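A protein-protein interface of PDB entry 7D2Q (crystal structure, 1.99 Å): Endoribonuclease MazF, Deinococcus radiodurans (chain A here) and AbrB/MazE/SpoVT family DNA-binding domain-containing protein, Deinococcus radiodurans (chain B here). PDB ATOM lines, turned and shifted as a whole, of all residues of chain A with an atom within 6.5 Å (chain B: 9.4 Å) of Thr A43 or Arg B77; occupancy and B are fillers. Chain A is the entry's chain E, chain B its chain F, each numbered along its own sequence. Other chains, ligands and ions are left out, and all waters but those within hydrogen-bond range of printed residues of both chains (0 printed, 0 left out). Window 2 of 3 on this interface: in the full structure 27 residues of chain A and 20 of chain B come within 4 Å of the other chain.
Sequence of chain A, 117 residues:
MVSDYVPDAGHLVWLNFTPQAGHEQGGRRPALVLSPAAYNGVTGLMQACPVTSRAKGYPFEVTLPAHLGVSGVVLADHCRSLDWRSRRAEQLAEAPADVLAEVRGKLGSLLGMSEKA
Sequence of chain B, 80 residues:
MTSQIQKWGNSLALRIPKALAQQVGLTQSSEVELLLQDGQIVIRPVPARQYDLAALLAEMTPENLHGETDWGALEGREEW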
ATOM      1  N   ALA A  38     -11.113   7.505  -3.070  1.00  0.00           N
ATOM      2  CA  ALA A  38     -11.956   6.749  -4.000  1.00  0.00           C
ATOM      3  C   ALA A  38     -12.351   7.604  -5.199  1.00  0.00           C
ATOM      4  O   ALA A  38     -12.209   7.190  -6.359  1.00  0.00           O
ATOM      5  CB  ALA A  38     -13.201   6.238  -3.273  1.00  0.00           C
ATOM      6  N   TYR A  39     -12.822   8.822  -4.924  1.00  0.00           N
ATOM      7  CA  TYR A  39     -13.141   9.782  -5.973  1.00  0.00           C
ATOM      8  C   TYR A  39     -11.881  10.293  -6.664  1.00  0.00           C
ATOM      9  O   TYR A  39     -11.826  10.362  -7.900  1.00  0.00           O
ATOM     10  CB  TYR A  39     -13.937  10.948  -5.369  1.00  0.00           C
ATOM     11  CG  TYR A  39     -14.178  12.096  -6.322  1.00  0.00           C
ATOM     12  CD1 TYR A  39     -15.269  12.088  -7.181  1.00  0.00           C
ATOM     13  CD2 TYR A  39     -13.330  13.188  -6.361  1.00  0.00           C
ATOM     14  CE1 TYR A  39     -15.506  13.130  -8.053  1.00  0.00           C
ATOM     15  CE2 TYR A  39     -13.559  14.240  -7.250  1.00  0.00           C
ATOM     16  CZ  TYR A  39     -14.648  14.198  -8.087  1.00  0.00           C
ATOM     17  OH  TYR A  39     -14.891  15.237  -8.968  1.00  0.00           O
ATOM     18  N   ASN A  40     -10.866  10.681  -5.879  1.00  0.00           N
ATOM     19  CA  ASN A  40      -9.690  11.344  -6.444  1.00  0.00           C
ATOM     20  C   ASN A  40      -8.967  10.438  -7.429  1.00  0.00           C
ATOM     21  O   ASN A  40      -8.578  10.871  -8.519  1.00  0.00           O
ATOM     22  CB  ASN A  40      -8.722  11.769  -5.339  1.00  0.00           C
ATOM     23  CG  ASN A  40      -9.379  12.638  -4.284  1.00  0.00           C
ATOM     24  OD1 ASN A  40     -10.373  13.313  -4.551  1.00  0.00           O
ATOM     25  ND2 ASN A  40      -8.827  12.623  -3.078  1.00  0.00           N
ATOM     26  N   GLY A  41      -8.766   9.178  -7.048  1.00  0.00           N
ATOM     27  CA  GLY A  41      -8.071   8.252  -7.927  1.00  0.00           C
ATOM     28  C   GLY A  41      -8.811   8.028  -9.228  1.00  0.00           C
ATOM     29  O   GLY A  41      -8.225   8.099 -10.310  1.00  0.00           O
ATOM     30  N   VAL A  42     -10.123   7.790  -9.140  1.00  0.00           N
ATOM     31  CA  VAL A  42     -10.897   7.457 -10.329  1.00  0.00           C
ATOM     32  C   VAL A  42     -10.952   8.644 -11.281  1.00  0.00           C
ATOM     33  O   VAL A  42     -10.637   8.516 -12.466  1.00  0.00           O
ATOM     34  CB  VAL A  42     -12.304   6.974  -9.931  1.00  0.00           C
ATOM     35  CG1 VAL A  42     -13.190   6.810 -11.158  1.00  0.00           C
ATOM     36  CG2 VAL A  42     -12.210   5.666  -9.166  1.00  0.00           C
ATOM     37  N   THR A  43     -11.321   9.827 -10.776  1.00  0.00           N
ATOM     38  CA  THR A  43     -11.622  10.958 -11.649  1.00  0.00           C
ATOM     39  C   THR A  43     -10.386  11.733 -12.095  1.00  0.00           C
ATOM     40  O   THR A  43     -10.451  12.447 -13.101  1.00  0.00           O
ATOM     41  CB  THR A  43     -12.563  11.948 -10.942  1.00  0.00           C
ATOM     42  OG1 THR A  43     -11.900  12.489  -9.786  1.00  0.00           O
ATOM     43  CG2 THR A  43     -13.844  11.259 -10.504  1.00  0.00           C
ATOM     44  N   GLY A  44      -9.287  11.655 -11.354  1.00  0.00           N
ATOM     45  CA  GLY A  44      -8.193  12.579 -11.565  1.00  0.00           C
ATOM     46  C   GLY A  44      -8.445  13.979 -11.045  1.00  0.00           C
ATOM     47  O   GLY A  44      -7.607  14.865 -11.251  1.00  0.00           O
ATOM     48  N   LEU A  45      -9.572  14.209 -10.389  1.00  0.00           N
ATOM     49  CA  LEU A  45      -9.914  15.496  -9.814  1.00  0.00           C
ATOM     50  C   LEU A  45     -10.001  15.351  -8.309  1.00  0.00           C
ATOM     51  O   LEU A  45     -10.071  14.239  -7.777  1.00  0.00           O
ATOM     52  CB  LEU A  45     -11.249  16.013 -10.360  1.00  0.00           C
ATOM     53  CG  LEU A  45     -11.362  16.284 -11.860  1.00  0.00           C
ATOM     54  CD1 LEU A  45     -12.809  16.551 -12.231  1.00  0.00           C
ATOM     55  CD2 LEU A  45     -10.493  17.457 -12.244  1.00  0.00           C
ATOM     56  N   MET A  46     -10.031  16.498  -7.629  1.00  0.00           N
ATOM     57  CA  MET A  46     -10.193  16.510  -6.183  1.00  0.00           C
ATOM     58  C   MET A  46     -10.714  17.874  -5.762  1.00  0.00           C
ATOM     59  O   MET A  46     -10.504  18.876  -6.448  1.00  0.00           O
ATOM     60  CB  MET A  46      -8.876  16.200  -5.465  1.00  0.00           C
ATOM     61  CG  MET A  46      -7.827  17.297  -5.634  1.00  0.00           C
ATOM     62  SD  MET A  46      -6.369  17.057  -4.596  1.00  0.00           S
ATOM     63  CE  MET A  46      -5.526  18.588  -4.850  1.00  0.00           C
ATOM     64  N   SER A  81     -12.478  22.441  -7.190  1.00  0.00           N
ATOM     65  CA  SER A  81     -12.100  21.229  -7.901  1.00  0.00           C
ATOM     66  C   SER A  81     -10.805  21.476  -8.662  1.00  0.00           C
ATOM     67  O   SER A  81     -10.688  22.470  -9.379  1.00  0.00           O
ATOM     68  CB  SER A  81     -13.211  20.806  -8.859  1.00  0.00           C
ATOM     69  OG  SER A  81     -12.765  19.767  -9.713  1.00  0.00           O
ATOM     70  N   ASP A  83      -7.430  19.455 -10.882  1.00  0.00           N
ATOM     71  CA  ASP A  83      -6.862  18.259 -11.509  1.00  0.00           C
ATOM     72  C   ASP A  83      -5.516  17.980 -10.854  1.00  0.00           C
ATOM     73  O   ASP A  83      -4.496  18.553 -11.236  1.00  0.00           O
ATOM     74  CB  ASP A  83      -6.720  18.445 -13.018  1.00  0.00           C
ATOM     75  CG  ASP A  83      -6.188  17.188 -13.738  1.00  0.00           C
ATOM     76  OD1 ASP A  83      -5.416  16.398 -13.149  1.00  0.00           O
ATOM     77  OD2 ASP A  83      -6.546  16.996 -14.918  1.00  0.00           O
ATOM     78  N   TRP A  84      -5.498  17.081  -9.871  1.00  0.00           N
ATOM     79  CA  TRP A  84      -4.254  16.847  -9.143  1.00  0.00           C
ATOM     80  C   TRP A  84      -3.224  16.090  -9.970  1.00  0.00           C
ATOM     81  O   TRP A  84      -2.023  16.235  -9.716  1.00  0.00           O
ATOM     82  CB  TRP A  84      -4.530  16.106  -7.838  1.00  0.00           C
ATOM     83  CG  TRP A  84      -5.171  14.769  -7.997  1.00  0.00           C
ATOM     84  CD1 TRP A  84      -6.509  14.492  -8.000  1.00  0.00           C
ATOM     85  CD2 TRP A  84      -4.500  13.515  -8.150  1.00  0.00           C
ATOM     86  NE1 TRP A  84      -6.712  13.137  -8.135  1.00  0.00           N
ATOM     87  CE2 TRP A  84      -5.493  12.517  -8.237  1.00  0.00           C
ATOM     88  CE3 TRP A  84      -3.155  13.139  -8.225  1.00  0.00           C
ATOM     89  CZ2 TRP A  84      -5.182  11.168  -8.395  1.00  0.00           C
ATOM     90  CZ3 TRP A  84      -2.848  11.797  -8.373  1.00  0.00           C
ATOM     91  CH2 TRP A  84      -3.857  10.831  -8.464  1.00  0.00           C
ATOM     92  N   ARG A  85      -3.653  15.311 -10.968  1.00  0.00           N
ATOM     93  CA  ARG A  85      -2.693  14.636 -11.838  1.00  0.00           C
ATOM     94  C   ARG A  85      -1.866  15.648 -12.625  1.00  0.00           C
ATOM     95  O   ARG A  85      -0.633  15.653 -12.547  1.00  0.00           O
ATOM     96  CB  ARG A  85      -3.415  13.671 -12.781  1.00  0.00           C
ATOM     97  CG  ARG A  85      -4.213  12.600 -12.072  1.00  0.00           C
ATOM     98  CD  ARG A  85      -4.302  11.310 -12.890  1.00  0.00           C
ATOM     99  NE  ARG A  85      -4.310  10.159 -11.997  1.00  0.00           N
ATOM    100  CZ  ARG A  85      -5.385   9.428 -11.733  1.00  0.00           C
ATOM    101  NH1 ARG A  85      -6.545   9.716 -12.320  1.00  0.00           N
ATOM    102  NH2 ARG A  85      -5.305   8.409 -10.883  1.00  0.00           N
ATOM    103  N   SER A  86      -2.533  16.539 -13.365  1.00  0.00           N
ATOM    104  CA  SER A  86      -1.810  17.531 -14.163  1.00  0.00           C
ATOM    105  C   SER A  86      -0.997  18.479 -13.303  1.00  0.00           C
ATOM    106  O   SER A  86       0.063  18.948 -13.731  1.00  0.00           O
ATOM    107  CB  SER A  86      -2.777  18.349 -15.028  1.00  0.00           C
ATOM    108  OG  SER A  86      -3.716  17.517 -15.678  1.00  0.00           O
ATOM    109  N   LEU B  74      -6.352  27.041 -16.193  1.00  0.00           N
ATOM    110  CA  LEU B  74      -7.025  25.759 -16.057  1.00  0.00           C
ATOM    111  C   LEU B  74      -6.126  24.654 -16.591  1.00  0.00           C
ATOM    112  O   LEU B  74      -5.413  24.838 -17.579  1.00  0.00           O
ATOM    113  CB  LEU B  74      -8.357  25.781 -16.802  1.00  0.00           C
ATOM    114  CG  LEU B  74      -9.248  26.941 -16.345  1.00  0.00           C
ATOM    115  CD1 LEU B  74     -10.600  26.949 -17.064  1.00  0.00           C
ATOM    116  CD2 LEU B  74      -9.428  26.903 -14.827  1.00  0.00           C
ATOM    117  N   GLU B  75      -6.145  23.507 -15.920  1.00  0.00           N
ATOM    118  CA  GLU B  75      -5.275  22.392 -16.259  1.00  0.00           C
ATOM    119  C   GLU B  75      -6.095  21.118 -16.360  1.00  0.00           C
ATOM    120  O   GLU B  75      -7.020  20.906 -15.574  1.00  0.00           O
ATOM    121  CB  GLU B  75      -4.163  22.207 -15.211  1.00  0.00           C
ATOM    122  CG  GLU B  75      -3.289  23.432 -14.987  1.00  0.00           C
ATOM    123  CD  GLU B  75      -1.851  23.070 -14.651  1.00  0.00           C
ATOM    124  OE1 GLU B  75      -1.507  21.868 -14.754  1.00  0.00           O
ATOM    125  OE2 GLU B  75      -1.068  23.981 -14.283  1.00  0.00           O
ATOM    126  N   GLY B  76      -5.762  20.287 -17.341  1.00  0.00           N
ATOM    127  CA  GLY B  76      -6.310  18.940 -17.402  1.00  0.00           C
ATOM    128  C   GLY B  76      -7.828  18.891 -17.456  1.00  0.00           C
ATOM    129  O   GLY B  76      -8.476  19.577 -18.257  1.00  0.00           O
ATOM    130  N   ARG B  77      -8.407  18.052 -16.595  1.00  0.00           N
ATOM    131  CA  ARG B  77      -9.845  17.820 -16.585  1.00  0.00           C
ATOM    132  C   ARG B  77     -10.616  18.893 -15.824  1.00  0.00           C
ATOM    133  O   ARG B  77     -11.836  18.749 -15.652  1.00  0.00           O
ATOM    134  CB  ARG B  77     -10.154  16.442 -15.992  1.00  0.00           C
ATOM    135  CG  ARG B  77      -9.920  15.270 -16.940  1.00  0.00           C
ATOM    136  CD  ARG B  77      -9.595  14.003 -16.151  1.00  0.00           C
ATOM    137  NE  ARG B  77      -8.488  14.250 -15.223  1.00  0.00           N
ATOM    138  CZ  ARG B  77      -7.333  13.584 -15.213  1.00  0.00           C
ATOM    139  NH1 ARG B  77      -7.111  12.592 -16.072  1.00  0.00           N
ATOM    140  NH2 ARG B  77      -6.400  13.912 -14.327  1.00  0.00           N
ATOM    141  N   GLU B  78      -9.938  19.942 -15.349  1.00  0.00           N
ATOM    142  CA  GLU B  78     -10.623  21.090 -14.763  1.00  0.00           C
ATOM    143  C   GLU B  78     -11.483  21.750 -15.823  1.00  0.00           C
ATOM    144  O   GLU B  78     -10.974  22.204 -16.851  1.00  0.00           O
ATOM    145  CB  GLU B  78      -9.616  22.096 -14.201  1.00  0.00           C
ATOM    146  CG  GLU B  78      -8.948  21.667 -12.898  1.00  0.00           C
ATOM    147  CD  GLU B  78      -7.678  22.445 -12.587  1.00  0.00           C
ATOM    148  OE1 GLU B  78      -6.817  21.897 -11.874  1.00  0.00           O
ATOM    149  OE2 GLU B  78      -7.538  23.604 -13.041  1.00  0.00           O
ATOM    150  N   GLU B  79     -12.789  21.811 -15.577  1.00  0.00           N
ATOM    151  CA  GLU B  79     -13.680  22.284 -16.625  1.00  0.00           C
ATOM    152  C   GLU B  79     -13.779  23.804 -16.651  1.00  0.00           C
ATOM    153  O   GLU B  79     -14.031  24.381 -17.714  1.00  0.00           O
ATOM    154  CB  GLU B  79     -15.059  21.647 -16.460  1.00  0.00           C
ATOM    155  CG  GLU B  79     -15.876  21.616 -17.741  1.00  0.00           C
ATOM    156  CD  GLU B  79     -17.296  22.047 -17.489  1.00  0.00           C
ATOM    157  OE1 GLU B  79     -18.098  22.137 -18.449  1.00  0.00           O
ATOM    158  OE2 GLU B  79     -17.601  22.292 -16.304  1.00  0.00           O
ATOM    159  N   TRP B  80     -13.557  24.469 -15.522  1.00  0.00           N
ATOM    160  CA  TRP B  80     -13.665  25.920 -15.483  1.00  0.00           C
ATOM    161  C   TRP B  80     -12.876  26.530 -14.324  1.00  0.00           C
ATOM    162  O   TRP B  80     -12.999  27.725 -14.035  1.00  0.00           O
ATOM    163  CB  TRP B  80     -15.138  26.331 -15.399  1.00  0.00           C
ATOM    164  CG  TRP B  80     -15.736  26.154 -14.036  1.00  0.00           C
ATOM    165  CD1 TRP B  80     -15.408  25.203 -13.106  1.00  0.00           C
ATOM    166  CD2 TRP B  80     -16.774  26.953 -13.448  1.00  0.00           C
ATOM    167  NE1 TRP B  80     -16.178  25.371 -11.972  1.00  0.00           N
ATOM    168  CE2 TRP B  80     -17.019  26.436 -12.156  1.00  0.00           C
ATOM    169  CE3 TRP B  80     -17.510  28.059 -13.885  1.00  0.00           C
ATOM    170  CZ2 TRP B  80     -17.975  26.979 -11.307  1.00  0.00           C
ATOM    171  CZ3 TRP B  80     -18.453  28.600 -13.039  1.00  0.00           C
ATOM    172  CH2 TRP B  80     -18.681  28.061 -11.764  1.00  0.00           C
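The backbone carbonyl oxygen (O) of Thr A43 lies within hydrogen-bond range of the guanidinium group (NE) of Arg B77 (3.4 Å).
The backbone carbonyl oxygen (O) of Ser A86 sits close to the side-chain carboxylate (OE1) of Glu B75.
The backbone NH of Asp A83 lies within hydrogen-bond range of the side-chain carboxylate of Glu B78.
NH2 of Arg B77 lies within salt-bridge range of OD1 of Asp A83 (2.9 Å).
O of Gly A44 is in hydrogen-bond range of NH2 of Arg B77, 3.4 Å away.
Ala A38 touches none of the printed residues of chain B.
Tyr A39 touches none of the printed residues of chain B.
No residue of chain B comes within 4 Å of Gly A41.
No residue of chain B comes within 4 Å of Val A42.
Thr A43 touches just one residue of chain B: Arg B77.
Of the printed residues of chain B, Gly A44 touches Arg B77.
Of the printed residues of chain B, Leu A45 touches Arg B77 (3.9 Å).
Printed residues of chain B within 4 Å of Arg A85: Arg B77 (3.4 Å).
Of the printed residues of chain B, Ser A86 touches Glu B75 and Gly B76.
Of the printed residues of chain A, Glu B75 touches Asp A83 (3.6 Å) and Ser A86 (3.5 Å).
Of chain A, only Thr A43 (3.4 Å), Gly A44 (3.4 Å), Leu A45 (3.9 Å), Asp A83 (2.7 Å) and Arg A85 (3.4 Å) come within 4 Å of Arg B77.
The nearest residue of chain A that does not touch Arg B77 is Ser A86 (4.7 Å).
Leu A45 touches Arg B77 (CD2 to C, 3.9 Å).
Asp A83 touches Glu B75 (CB to O, 3.6 Å).
Gly B76 touches Asp A83.
Arg B77 touches Arg A85.
Ser A86 touches Gly B76 (OG to CA, 3.4 Å).
The side-chain hydroxyl (OG1) of Thr A43 sits at hydrogen-bond distance from the backbone NH (N) of Leu A45 (3.0 Å).
O of Leu A45 lies close to OD1 of Asn A40.
O of Gly A44 lies within hydrogen-bond range of N of Trp A84, 3.4 Å away.
N of Glu B75 sits at hydrogen-bond distance from OE2 of Glu B78.
The backbone NH (N) of Ser A86 sits at hydrogen-bond distance from the side-chain carboxylate (OD1) of Asp A83 (2.9 Å).
OG1 of Thr A43 is in hydrogen-bond range of O of Tyr A39 (2.8 Å).
Of the 7 printed residues of chain B, 4 touch a printed residue of chain A.
Hydrophobic or aromatic side chains of chain A that line the printed part of chain B: Leu A45.
Among the printed residues, Asp or Glu carboxylates within 4 Å of a Lys or Arg side-chain nitrogen of the other chain: Asp A83 with Arg B77 (2.9 Å).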
